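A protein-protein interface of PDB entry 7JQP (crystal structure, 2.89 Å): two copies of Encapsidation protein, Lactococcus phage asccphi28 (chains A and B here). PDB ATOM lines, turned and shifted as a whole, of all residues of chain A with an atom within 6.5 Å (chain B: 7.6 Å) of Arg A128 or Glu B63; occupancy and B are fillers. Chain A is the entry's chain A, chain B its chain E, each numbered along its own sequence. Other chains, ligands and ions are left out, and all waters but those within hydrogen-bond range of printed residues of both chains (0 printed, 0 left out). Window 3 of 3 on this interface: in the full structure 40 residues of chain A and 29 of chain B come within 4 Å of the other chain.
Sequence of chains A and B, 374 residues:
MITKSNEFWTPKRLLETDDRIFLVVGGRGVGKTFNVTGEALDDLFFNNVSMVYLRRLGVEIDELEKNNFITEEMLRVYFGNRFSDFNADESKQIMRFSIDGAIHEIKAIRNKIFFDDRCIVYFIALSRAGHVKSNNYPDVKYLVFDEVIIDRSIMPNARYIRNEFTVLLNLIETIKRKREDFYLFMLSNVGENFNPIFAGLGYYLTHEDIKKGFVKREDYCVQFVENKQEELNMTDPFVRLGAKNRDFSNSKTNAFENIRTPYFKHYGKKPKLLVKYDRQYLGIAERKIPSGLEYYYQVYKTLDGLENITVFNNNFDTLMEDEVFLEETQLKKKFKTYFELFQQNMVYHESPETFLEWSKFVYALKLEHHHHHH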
ATOM      1  N   ARG A  56      17.413 -27.849 -31.556  1.00  0.00           N
ATOM      2  CA  ARG A  56      18.464 -28.376 -30.695  1.00  0.00           C
ATOM      3  C   ARG A  56      19.735 -27.539 -30.777  1.00  0.00           C
ATOM      4  O   ARG A  56      20.363 -27.256 -29.751  1.00  0.00           O
ATOM      5  CB  ARG A  56      18.771 -29.832 -31.047  1.00  0.00           C
ATOM      6  CG  ARG A  56      19.755 -30.471 -30.079  1.00  0.00           C
ATOM      7  CD  ARG A  56      19.861 -31.973 -30.258  1.00  0.00           C
ATOM      8  NE  ARG A  56      18.784 -32.688 -29.582  1.00  0.00           N
ATOM      9  CZ  ARG A  56      17.688 -33.146 -30.178  1.00  0.00           C
ATOM     10  NH1 ARG A  56      17.505 -32.976 -31.482  1.00  0.00           N
ATOM     11  NH2 ARG A  56      16.773 -33.784 -29.465  1.00  0.00           N
ATOM     12  N   LEU A  57      20.137 -27.138 -31.981  1.00  0.00           N
ATOM     13  CA  LEU A  57      21.418 -26.480 -32.187  1.00  0.00           C
ATOM     14  C   LEU A  57      21.234 -25.095 -32.789  1.00  0.00           C
ATOM     15  O   LEU A  57      20.257 -24.828 -33.495  1.00  0.00           O
ATOM     16  CB  LEU A  57      22.321 -27.316 -33.102  1.00  0.00           C
ATOM     17  CG  LEU A  57      22.731 -28.687 -32.565  1.00  0.00           C
ATOM     18  CD1 LEU A  57      23.486 -29.466 -33.627  1.00  0.00           C
ATOM     19  CD2 LEU A  57      23.568 -28.536 -31.305  1.00  0.00           C
ATOM     20  N   GLY A  58      22.198 -24.218 -32.503  1.00  0.00           N
ATOM     21  CA  GLY A  58      22.124 -22.863 -33.020  1.00  0.00           C
ATOM     22  C   GLY A  58      22.131 -22.812 -34.534  1.00  0.00           C
ATOM     23  O   GLY A  58      21.419 -22.008 -35.141  1.00  0.00           O
ATOM     24  N   VAL A  59      22.930 -23.675 -35.168  1.00  0.00           N
ATOM     25  CA  VAL A  59      23.001 -23.679 -36.625  1.00  0.00           C
ATOM     26  C   VAL A  59      21.626 -23.940 -37.226  1.00  0.00           C
ATOM     27  O   VAL A  59      21.274 -23.387 -38.276  1.00  0.00           O
ATOM     28  CB  VAL A  59      24.030 -24.720 -37.107  1.00  0.00           C
ATOM     29  CG1 VAL A  59      25.406 -24.415 -36.535  1.00  0.00           C
ATOM     30  CG2 VAL A  59      23.583 -26.127 -36.724  1.00  0.00           C
ATOM     31  N   ILE A  61      18.857 -22.840 -36.273  1.00  0.00           N
ATOM     32  CA  ILE A  61      18.128 -21.575 -36.316  1.00  0.00           C
ATOM     33  C   ILE A  61      18.858 -20.539 -37.155  1.00  0.00           C
ATOM     34  O   ILE A  61      18.227 -19.784 -37.898  1.00  0.00           O
ATOM     35  CB  ILE A  61      17.879 -21.072 -34.877  1.00  0.00           C
ATOM     36  CG1 ILE A  61      16.806 -21.959 -34.238  1.00  0.00           C
ATOM     37  CG2 ILE A  61      17.482 -19.605 -34.865  1.00  0.00           C
ATOM     38  CD1 ILE A  61      16.408 -21.551 -32.866  1.00  0.00           C
ATOM     39  N   ASP A  62      20.184 -20.471 -37.043  1.00  0.00           N
ATOM     40  CA  ASP A  62      20.929 -19.492 -37.825  1.00  0.00           C
ATOM     41  C   ASP A  62      20.710 -19.711 -39.316  1.00  0.00           C
ATOM     42  O   ASP A  62      20.565 -18.747 -40.079  1.00  0.00           O
ATOM     43  CB  ASP A  62      22.413 -19.562 -37.471  1.00  0.00           C
ATOM     44  CG  ASP A  62      22.711 -18.992 -36.094  1.00  0.00           C
ATOM     45  OD1 ASP A  62      21.816 -18.349 -35.502  1.00  0.00           O
ATOM     46  OD2 ASP A  62      23.841 -19.183 -35.601  1.00  0.00           O
ATOM     47  N   ASN A 111      16.064 -12.993 -34.417  1.00  0.00           N
ATOM     48  CA  ASN A 111      15.468 -14.240 -33.967  1.00  0.00           C
ATOM     49  C   ASN A 111      14.013 -14.077 -33.554  1.00  0.00           C
ATOM     50  O   ASN A 111      13.488 -14.924 -32.823  1.00  0.00           O
ATOM     51  CB  ASN A 111      16.300 -14.786 -32.803  1.00  0.00           C
ATOM     52  CG  ASN A 111      17.528 -15.556 -33.263  1.00  0.00           C
ATOM     53  OD1 ASN A 111      17.823 -15.623 -34.457  1.00  0.00           O
ATOM     54  ND2 ASN A 111      18.305 -16.052 -32.304  1.00  0.00           N
ATOM     55  N   PHE A 123      12.690 -17.563 -31.668  1.00  0.00           N
ATOM     56  CA  PHE A 123      13.557 -18.658 -32.081  1.00  0.00           C
ATOM     57  C   PHE A 123      14.643 -18.846 -31.031  1.00  0.00           C
ATOM     58  O   PHE A 123      15.360 -17.899 -30.694  1.00  0.00           O
ATOM     59  CB  PHE A 123      14.151 -18.375 -33.462  1.00  0.00           C
ATOM     60  CG  PHE A 123      13.115 -18.330 -34.558  1.00  0.00           C
ATOM     61  CD1 PHE A 123      12.695 -19.491 -35.185  1.00  0.00           C
ATOM     62  CD2 PHE A 123      12.546 -17.126 -34.943  1.00  0.00           C
ATOM     63  CE1 PHE A 123      11.738 -19.452 -36.183  1.00  0.00           C
ATOM     64  CE2 PHE A 123      11.589 -17.083 -35.941  1.00  0.00           C
ATOM     65  CZ  PHE A 123      11.183 -18.248 -36.560  1.00  0.00           C
ATOM     66  N   ILE A 124      14.740 -20.069 -30.506  1.00  0.00           N
ATOM     67  CA  ILE A 124      15.660 -20.413 -29.432  1.00  0.00           C
ATOM     68  C   ILE A 124      16.351 -21.726 -29.756  1.00  0.00           C
ATOM     69  O   ILE A 124      15.768 -22.626 -30.367  1.00  0.00           O
ATOM     70  CB  ILE A 124      14.936 -20.564 -28.076  1.00  0.00           C
ATOM     71  CG1 ILE A 124      14.057 -19.364 -27.779  1.00  0.00           C
ATOM     72  CG2 ILE A 124      15.929 -20.859 -26.952  1.00  0.00           C
ATOM     73  CD1 ILE A 124      13.171 -19.614 -26.601  1.00  0.00           C
ATOM     74  N   ALA A 125      17.580 -21.856 -29.275  1.00  0.00           N
ATOM     75  CA  ALA A 125      18.374 -23.060 -29.456  1.00  0.00           C
ATOM     76  C   ALA A 125      18.637 -23.685 -28.095  1.00  0.00           C
ATOM     77  O   ALA A 125      19.057 -22.996 -27.159  1.00  0.00           O
ATOM     78  CB  ALA A 125      19.693 -22.742 -30.164  1.00  0.00           C
ATOM     79  N   LEU A 126      18.370 -24.985 -27.986  1.00  0.00           N
ATOM     80  CA  LEU A 126      18.557 -25.672 -26.714  1.00  0.00           C
ATOM     81  C   LEU A 126      20.001 -25.575 -26.246  1.00  0.00           C
ATOM     82  O   LEU A 126      20.260 -25.546 -25.039  1.00  0.00           O
ATOM     83  CB  LEU A 126      18.123 -27.127 -26.862  1.00  0.00           C
ATOM     84  CG  LEU A 126      17.671 -27.885 -25.617  1.00  0.00           C
ATOM     85  CD1 LEU A 126      16.700 -27.094 -24.768  1.00  0.00           C
ATOM     86  CD2 LEU A 126      17.044 -29.209 -26.065  1.00  0.00           C
ATOM     87  N   SER A 127      20.951 -25.506 -27.183  1.00  0.00           N
ATOM     88  CA  SER A 127      22.350 -25.338 -26.804  1.00  0.00           C
ATOM     89  C   SER A 127      22.557 -24.037 -26.039  1.00  0.00           C
ATOM     90  O   SER A 127      23.354 -23.982 -25.095  1.00  0.00           O
ATOM     91  CB  SER A 127      23.235 -25.361 -28.049  1.00  0.00           C
ATOM     92  OG  SER A 127      22.569 -25.989 -29.129  1.00  0.00           O
ATOM     93  N   ARG A 128      21.854 -22.980 -26.435  1.00  0.00           N
ATOM     94  CA  ARG A 128      21.966 -21.677 -25.798  1.00  0.00           C
ATOM     95  C   ARG A 128      20.906 -21.462 -24.726  1.00  0.00           C
ATOM     96  O   ARG A 128      20.835 -20.371 -24.150  1.00  0.00           O
ATOM     97  CB  ARG A 128      21.848 -20.577 -26.865  1.00  0.00           C
ATOM     98  CG  ARG A 128      22.633 -20.870 -28.142  1.00  0.00           C
ATOM     99  CD  ARG A 128      22.254 -19.929 -29.286  1.00  0.00           C
ATOM    100  NE  ARG A 128      23.078 -20.162 -30.472  1.00  0.00           N
ATOM    101  CZ  ARG A 128      22.804 -19.689 -31.686  1.00  0.00           C
ATOM    102  NH1 ARG A 128      21.719 -18.954 -31.890  1.00  0.00           N
ATOM    103  NH2 ARG A 128      23.617 -19.954 -32.700  1.00  0.00           N
ATOM    104  N   ALA A 129      20.093 -22.483 -24.442  1.00  0.00           N
ATOM    105  CA  ALA A 129      19.001 -22.338 -23.486  1.00  0.00           C
ATOM    106  C   ALA A 129      19.502 -22.107 -22.064  1.00  0.00           C
ATOM    107  O   ALA A 129      18.868 -21.380 -21.289  1.00  0.00           O
ATOM    108  CB  ALA A 129      18.105 -23.579 -23.538  1.00  0.00           C
ATOM    109  N   GLY A 130      20.615 -22.741 -21.692  1.00  0.00           N
ATOM    110  CA  GLY A 130      21.076 -22.655 -20.313  1.00  0.00           C
ATOM    111  C   GLY A 130      21.320 -21.238 -19.833  1.00  0.00           C
ATOM    112  O   GLY A 130      20.951 -20.881 -18.711  1.00  0.00           O
ATOM    113  N   HIS A 131      21.957 -20.414 -20.663  1.00  0.00           N
ATOM    114  CA  HIS A 131      22.250 -19.052 -20.239  1.00  0.00           C
ATOM    115  C   HIS A 131      21.011 -18.163 -20.187  1.00  0.00           C
ATOM    116  O   HIS A 131      21.038 -17.130 -19.507  1.00  0.00           O
ATOM    117  CB  HIS A 131      23.317 -18.397 -21.123  1.00  0.00           C
ATOM    118  CG  HIS A 131      24.630 -19.117 -21.121  1.00  0.00           C
ATOM    119  ND1 HIS A 131      25.462 -19.111 -20.022  1.00  0.00           N
ATOM    120  CD2 HIS A 131      25.281 -19.814 -22.083  1.00  0.00           C
ATOM    121  CE1 HIS A 131      26.555 -19.799 -20.295  1.00  0.00           C
ATOM    122  NE2 HIS A 131      26.471 -20.237 -21.539  1.00  0.00           N
ATOM    123  N   VAL A 132      19.926 -18.533 -20.862  1.00  0.00           N
ATOM    124  CA  VAL A 132      18.736 -17.691 -20.876  1.00  0.00           C
ATOM    125  C   VAL A 132      17.784 -18.133 -19.773  1.00  0.00           C
ATOM    126  O   VAL A 132      16.561 -18.008 -19.908  1.00  0.00           O
ATOM    127  CB  VAL A 132      18.022 -17.718 -22.242  1.00  0.00           C
ATOM    128  CG1 VAL A 132      18.987 -17.394 -23.363  1.00  0.00           C
ATOM    129  CG2 VAL A 132      17.379 -19.086 -22.471  1.00  0.00           C
ATOM    130  N   LYS A 133      18.330 -18.580 -18.642  1.00  0.00           N
ATOM    131  CA  LYS A 133      17.456 -19.040 -17.572  1.00  0.00           C
ATOM    132  C   LYS A 133      16.751 -17.861 -16.920  1.00  0.00           C
ATOM    133  O   LYS A 133      15.660 -18.021 -16.361  1.00  0.00           O
ATOM    134  CB  LYS A 133      18.261 -19.803 -16.517  1.00  0.00           C
ATOM    135  CG  LYS A 133      18.724 -21.181 -16.949  1.00  0.00           C
ATOM    136  N   ASN A 135      15.861 -15.141 -18.769  1.00  0.00           N
ATOM    137  CA  ASN A 135      15.119 -14.418 -19.795  1.00  0.00           C
ATOM    138  C   ASN A 135      13.626 -14.419 -19.485  1.00  0.00           C
ATOM    139  O   ASN A 135      13.104 -15.317 -18.817  1.00  0.00           O
ATOM    140  CB  ASN A 135      15.375 -15.033 -21.173  1.00  0.00           C
ATOM    141  CG  ASN A 135      16.664 -14.534 -21.801  1.00  0.00           C
ATOM    142  OD1 ASN A 135      17.473 -13.886 -21.141  1.00  0.00           O
ATOM    143  ND2 ASN A 135      16.859 -14.836 -23.079  1.00  0.00           N
ATOM    144  N   TYR A 137       9.743 -14.126 -21.154  1.00  0.00           N
ATOM    145  CA  TYR A 137       8.866 -14.281 -22.317  1.00  0.00           C
ATOM    146  C   TYR A 137       7.429 -14.069 -21.861  1.00  0.00           C
ATOM    147  O   TYR A 137       6.799 -15.004 -21.337  1.00  0.00           O
ATOM    148  CB  TYR A 137       9.030 -15.652 -22.965  1.00  0.00           C
ATOM    149  CG  TYR A 137      10.458 -15.972 -23.332  1.00  0.00           C
ATOM    150  CD1 TYR A 137      11.004 -15.527 -24.529  1.00  0.00           C
ATOM    151  CD2 TYR A 137      11.261 -16.717 -22.481  1.00  0.00           C
ATOM    152  CE1 TYR A 137      12.310 -15.819 -24.869  1.00  0.00           C
ATOM    153  CE2 TYR A 137      12.568 -17.015 -22.813  1.00  0.00           C
ATOM    154  CZ  TYR A 137      13.087 -16.562 -24.009  1.00  0.00           C
ATOM    155  OH  TYR A 137      14.389 -16.854 -24.346  1.00  0.00           O
ATOM    156  N   ILE A 161      22.368 -32.859 -26.537  1.00  0.00           N
ATOM    157  CA  ILE A 161      23.014 -32.021 -25.536  1.00  0.00           C
ATOM    158  C   ILE A 161      23.183 -32.810 -24.242  1.00  0.00           C
ATOM    159  O   ILE A 161      22.390 -33.707 -23.920  1.00  0.00           O
ATOM    160  CB  ILE A 161      22.211 -30.731 -25.296  1.00  0.00           C
ATOM    161  CG1 ILE A 161      21.923 -30.029 -26.623  1.00  0.00           C
ATOM    162  CG2 ILE A 161      22.974 -29.791 -24.370  1.00  0.00           C
ATOM    163  CD1 ILE A 161      20.962 -28.874 -26.504  1.00  0.00           C
ATOM    164  N   LEU B  57      29.948 -14.383 -18.851  1.00  0.00           N
ATOM    165  CA  LEU B  57      30.318 -14.578 -20.246  1.00  0.00           C
ATOM    166  C   LEU B  57      29.446 -13.731 -21.162  1.00  0.00           C
ATOM    167  O   LEU B  57      28.300 -13.404 -20.835  1.00  0.00           O
ATOM    168  CB  LEU B  57      30.215 -16.052 -20.646  1.00  0.00           C
ATOM    169  CG  LEU B  57      31.171 -17.004 -19.923  1.00  0.00           C
ATOM    170  CD1 LEU B  57      30.854 -18.445 -20.298  1.00  0.00           C
ATOM    171  CD2 LEU B  57      32.623 -16.665 -20.239  1.00  0.00           C
ATOM    172  N   GLY B  58      30.009 -13.379 -22.321  1.00  0.00           N
ATOM    173  CA  GLY B  58      29.294 -12.512 -23.243  1.00  0.00           C
ATOM    174  C   GLY B  58      27.991 -13.102 -23.754  1.00  0.00           C
ATOM    175  O   GLY B  58      26.974 -12.405 -23.816  1.00  0.00           O
ATOM    176  N   VAL B  59      27.991 -14.395 -24.100  1.00  0.00           N
ATOM    177  CA  VAL B  59      26.763 -15.004 -24.609  1.00  0.00           C
ATOM    178  C   VAL B  59      25.665 -14.941 -23.560  1.00  0.00           C
ATOM    179  O   VAL B  59      24.479 -14.832 -23.899  1.00  0.00           O
ATOM    180  CB  VAL B  59      26.986 -16.452 -25.085  1.00  0.00           C
ATOM    181  CG1 VAL B  59      27.719 -16.449 -26.420  1.00  0.00           C
ATOM    182  CG2 VAL B  59      27.721 -17.264 -24.037  1.00  0.00           C
ATOM    183  N   GLU B  60      26.025 -15.023 -22.275  1.00  0.00           N
ATOM    184  CA  GLU B  60      25.002 -14.881 -21.245  1.00  0.00           C
ATOM    185  C   GLU B  60      24.248 -13.578 -21.453  1.00  0.00           C
ATOM    186  O   GLU B  60      23.053 -13.488 -21.156  1.00  0.00           O
ATOM    187  CB  GLU B  60      25.619 -14.902 -19.847  1.00  0.00           C
ATOM    188  CG  GLU B  60      26.554 -16.068 -19.589  1.00  0.00           C
ATOM    189  CD  GLU B  60      26.655 -16.418 -18.114  1.00  0.00           C
ATOM    190  OE1 GLU B  60      25.611 -16.722 -17.500  1.00  0.00           O
ATOM    191  OE2 GLU B  60      27.777 -16.394 -17.569  1.00  0.00           O
ATOM    192  N   ILE B  61      24.938 -12.563 -21.968  1.00  0.00           N
ATOM    193  CA  ILE B  61      24.325 -11.288 -22.309  1.00  0.00           C
ATOM    194  C   ILE B  61      23.845 -11.268 -23.754  1.00  0.00           C
ATOM    195  O   ILE B  61      22.771 -10.742 -24.044  1.00  0.00           O
ATOM    196  CB  ILE B  61      25.329 -10.151 -22.018  1.00  0.00           C
ATOM    197  CG1 ILE B  61      25.456 -10.008 -20.497  1.00  0.00           C
ATOM    198  CG2 ILE B  61      24.898  -8.856 -22.669  1.00  0.00           C
ATOM    199  CD1 ILE B  61      26.338  -8.902 -20.050  1.00  0.00           C
ATOM    200  N   ASP B  62      24.624 -11.820 -24.685  1.00  0.00           N
ATOM    201  CA  ASP B  62      24.189 -11.825 -26.078  1.00  0.00           C
ATOM    202  C   ASP B  62      22.875 -12.581 -26.232  1.00  0.00           C
ATOM    203  O   ASP B  62      21.971 -12.136 -26.949  1.00  0.00           O
ATOM    204  CB  ASP B  62      25.268 -12.436 -26.971  1.00  0.00           C
ATOM    205  CG  ASP B  62      26.472 -11.529 -27.136  1.00  0.00           C
ATOM    206  OD1 ASP B  62      26.394 -10.346 -26.736  1.00  0.00           O
ATOM    207  OD2 ASP B  62      27.504 -12.003 -27.653  1.00  0.00           O
ATOM    208  N   GLU B  63      22.752 -13.726 -25.562  1.00  0.00           N
ATOM    209  CA  GLU B  63      21.507 -14.480 -25.566  1.00  0.00           C
ATOM    210  C   GLU B  63      20.458 -13.879 -24.643  1.00  0.00           C
ATOM    211  O   GLU B  63      19.289 -14.272 -24.722  1.00  0.00           O
ATOM    212  CB  GLU B  63      21.767 -15.933 -25.160  1.00  0.00           C
ATOM    213  CG  GLU B  63      22.525 -16.738 -26.204  1.00  0.00           C
ATOM    214  CD  GLU B  63      21.825 -16.756 -27.551  1.00  0.00           C
ATOM    215  OE1 GLU B  63      20.584 -16.901 -27.579  1.00  0.00           O
ATOM    216  OE2 GLU B  63      22.516 -16.609 -28.582  1.00  0.00           O
ATOM    217  N   LEU B  64      20.843 -12.950 -23.774  1.00  0.00           N
ATOM    218  CA  LEU B  64      19.885 -12.305 -22.886  1.00  0.00           C
ATOM    219  C   LEU B  64      18.918 -11.455 -23.697  1.00  0.00           C
ATOM    220  O   LEU B  64      19.297 -10.828 -24.690  1.00  0.00           O
ATOM    221  CB  LEU B  64      20.621 -11.445 -21.862  1.00  0.00           C
ATOM    222  CG  LEU B  64      19.812 -10.631 -20.851  1.00  0.00           C
ATOM    223  CD1 LEU B  64      19.077 -11.526 -19.875  1.00  0.00           C
ATOM    224  CD2 LEU B  64      20.743  -9.675 -20.111  1.00  0.00           C
ATOM    225  N   GLU B  65      17.658 -11.437 -23.268  1.00  0.00           N
ATOM    226  CA  GLU B  65      16.629 -10.627 -23.919  1.00  0.00           C
ATOM    227  C   GLU B  65      16.581  -9.282 -23.207  1.00  0.00           C
ATOM    228  O   GLU B  65      15.873  -9.104 -22.213  1.00  0.00           O
ATOM    229  CB  GLU B  65      15.285 -11.342 -23.883  1.00  0.00           C
ATOM    230  CG  GLU B  65      15.182 -12.523 -24.836  1.00  0.00           C
ATOM    231  CD  GLU B  65      14.935 -12.093 -26.269  1.00  0.00           C
ATOM    232  OE1 GLU B  65      14.195 -11.107 -26.471  1.00  0.00           O
ATOM    233  OE2 GLU B  65      15.475 -12.738 -27.191  1.00  0.00           O
ATOM    234  N   LYS B  66      17.347  -8.319 -23.731  1.00  0.00           N
ATOM    235  CA  LYS B  66      17.407  -7.006 -23.101  1.00  0.00           C
ATOM    236  C   LYS B  66      16.043  -6.325 -23.137  1.00  0.00           C
ATOM    237  O   LYS B  66      15.673  -5.599 -22.206  1.00  0.00           O
ATOM    238  CB  LYS B  66      18.425  -6.106 -23.807  1.00  0.00           C
ATOM    239  CG  LYS B  66      19.651  -6.748 -24.432  1.00  0.00           C
ATOM    240  CD  LYS B  66      20.695  -7.204 -23.439  1.00  0.00           C
ATOM    241  CE  LYS B  66      22.052  -7.298 -24.139  1.00  0.00           C
ATOM    242  NZ  LYS B  66      21.976  -8.033 -25.440  1.00  0.00           N
ATOM    243  N   ARG B 128      34.491  -9.119 -21.118  1.00  0.00           N
ATOM    244  CA  ARG B 128      34.646  -7.869 -21.845  1.00  0.00           C
ATOM    245  C   ARG B 128      34.892  -6.688 -20.914  1.00  0.00           C
ATOM    246  O   ARG B 128      34.885  -5.539 -21.371  1.00  0.00           O
ATOM    247  CB  ARG B 128      33.405  -7.614 -22.708  1.00  0.00           C
ATOM    248  CG  ARG B 128      32.921  -8.845 -23.473  1.00  0.00           C
ATOM    249  CD  ARG B 128      31.537  -8.641 -24.080  1.00  0.00           C
ATOM    250  NE  ARG B 128      31.135  -9.783 -24.900  1.00  0.00           N
ATOM    251  CZ  ARG B 128      29.895 -10.005 -25.326  1.00  0.00           C
ATOM    252  NH1 ARG B 128      28.917  -9.169 -25.004  1.00  0.00           N
ATOM    253  NH2 ARG B 128      29.631 -11.070 -26.071  1.00  0.00           N
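Of the 21 printed residues of chain A, 4 touch a printed residue of chain B. Hydrophobic or aromatic side chains of chain A that line the printed part of chain B: His A131 and Val A132. Among the printed residues, no Asp or Glu carboxylate lies within 4 Å of a Lys or Arg side-chain nitrogen of the other chain.
Of chain B, only Glu B63 (3.4 Å) comes within 4 Å of Arg A128. Of chain A, only Arg A128 (3.4 Å), Val A132 (3.4 Å) and Asn A135 (3.0 Å) come within 4 Å of Glu B63. Of the printed residues of chain B, Asn A135 touches Glu B63, Leu B64 and Glu B65. Of the printed residues of chain A, Glu B65 touches Asn A135. Arg B128 touches none of the printed residues of chain A. Asp A62 touches none of the printed residues of chain B. The nearest residue of chain B that does not touch Arg A128 is Val B59 (6.6 Å). The nearest residue of chain A that does not touch Glu B63 is His A131 (5.0 Å).
6 positions are printed for both chains. Of the 6 pairs that touch across the chains among the printed residues, none has its exchanged pair printed and touching as well.
The side-chain carboxylate (OD2) of Asp A62 lies within salt-bridge range of the guanidinium group (NH2) of Arg A128 (3.0 Å). The side-chain amide nitrogen (ND2) of Asn A135 lies within hydrogen-bond range of the side-chain hydroxyl (OH) of Tyr A137 (3.4 Å). N of Leu B57 sits at hydrogen-bond distance from OE2 of Glu B60 (3.2 Å).
Arg A128 touches Glu B63. Val A132 touches Glu B63 (CG1 to O, 3.4 Å). Asn A135 touches Leu B64.
N of Glu B65 lies within hydrogen-bond range of OD1 of Asn A135 (3.2 Å). ND1 of His A131 lies close to OE1 of Glu B60 (3.5 Å). The backbone carbonyl oxygen (O) of Glu B63 sits at hydrogen-bond distance from the side-chain amide nitrogen (ND2) of Asn A135 (3.0 Å).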
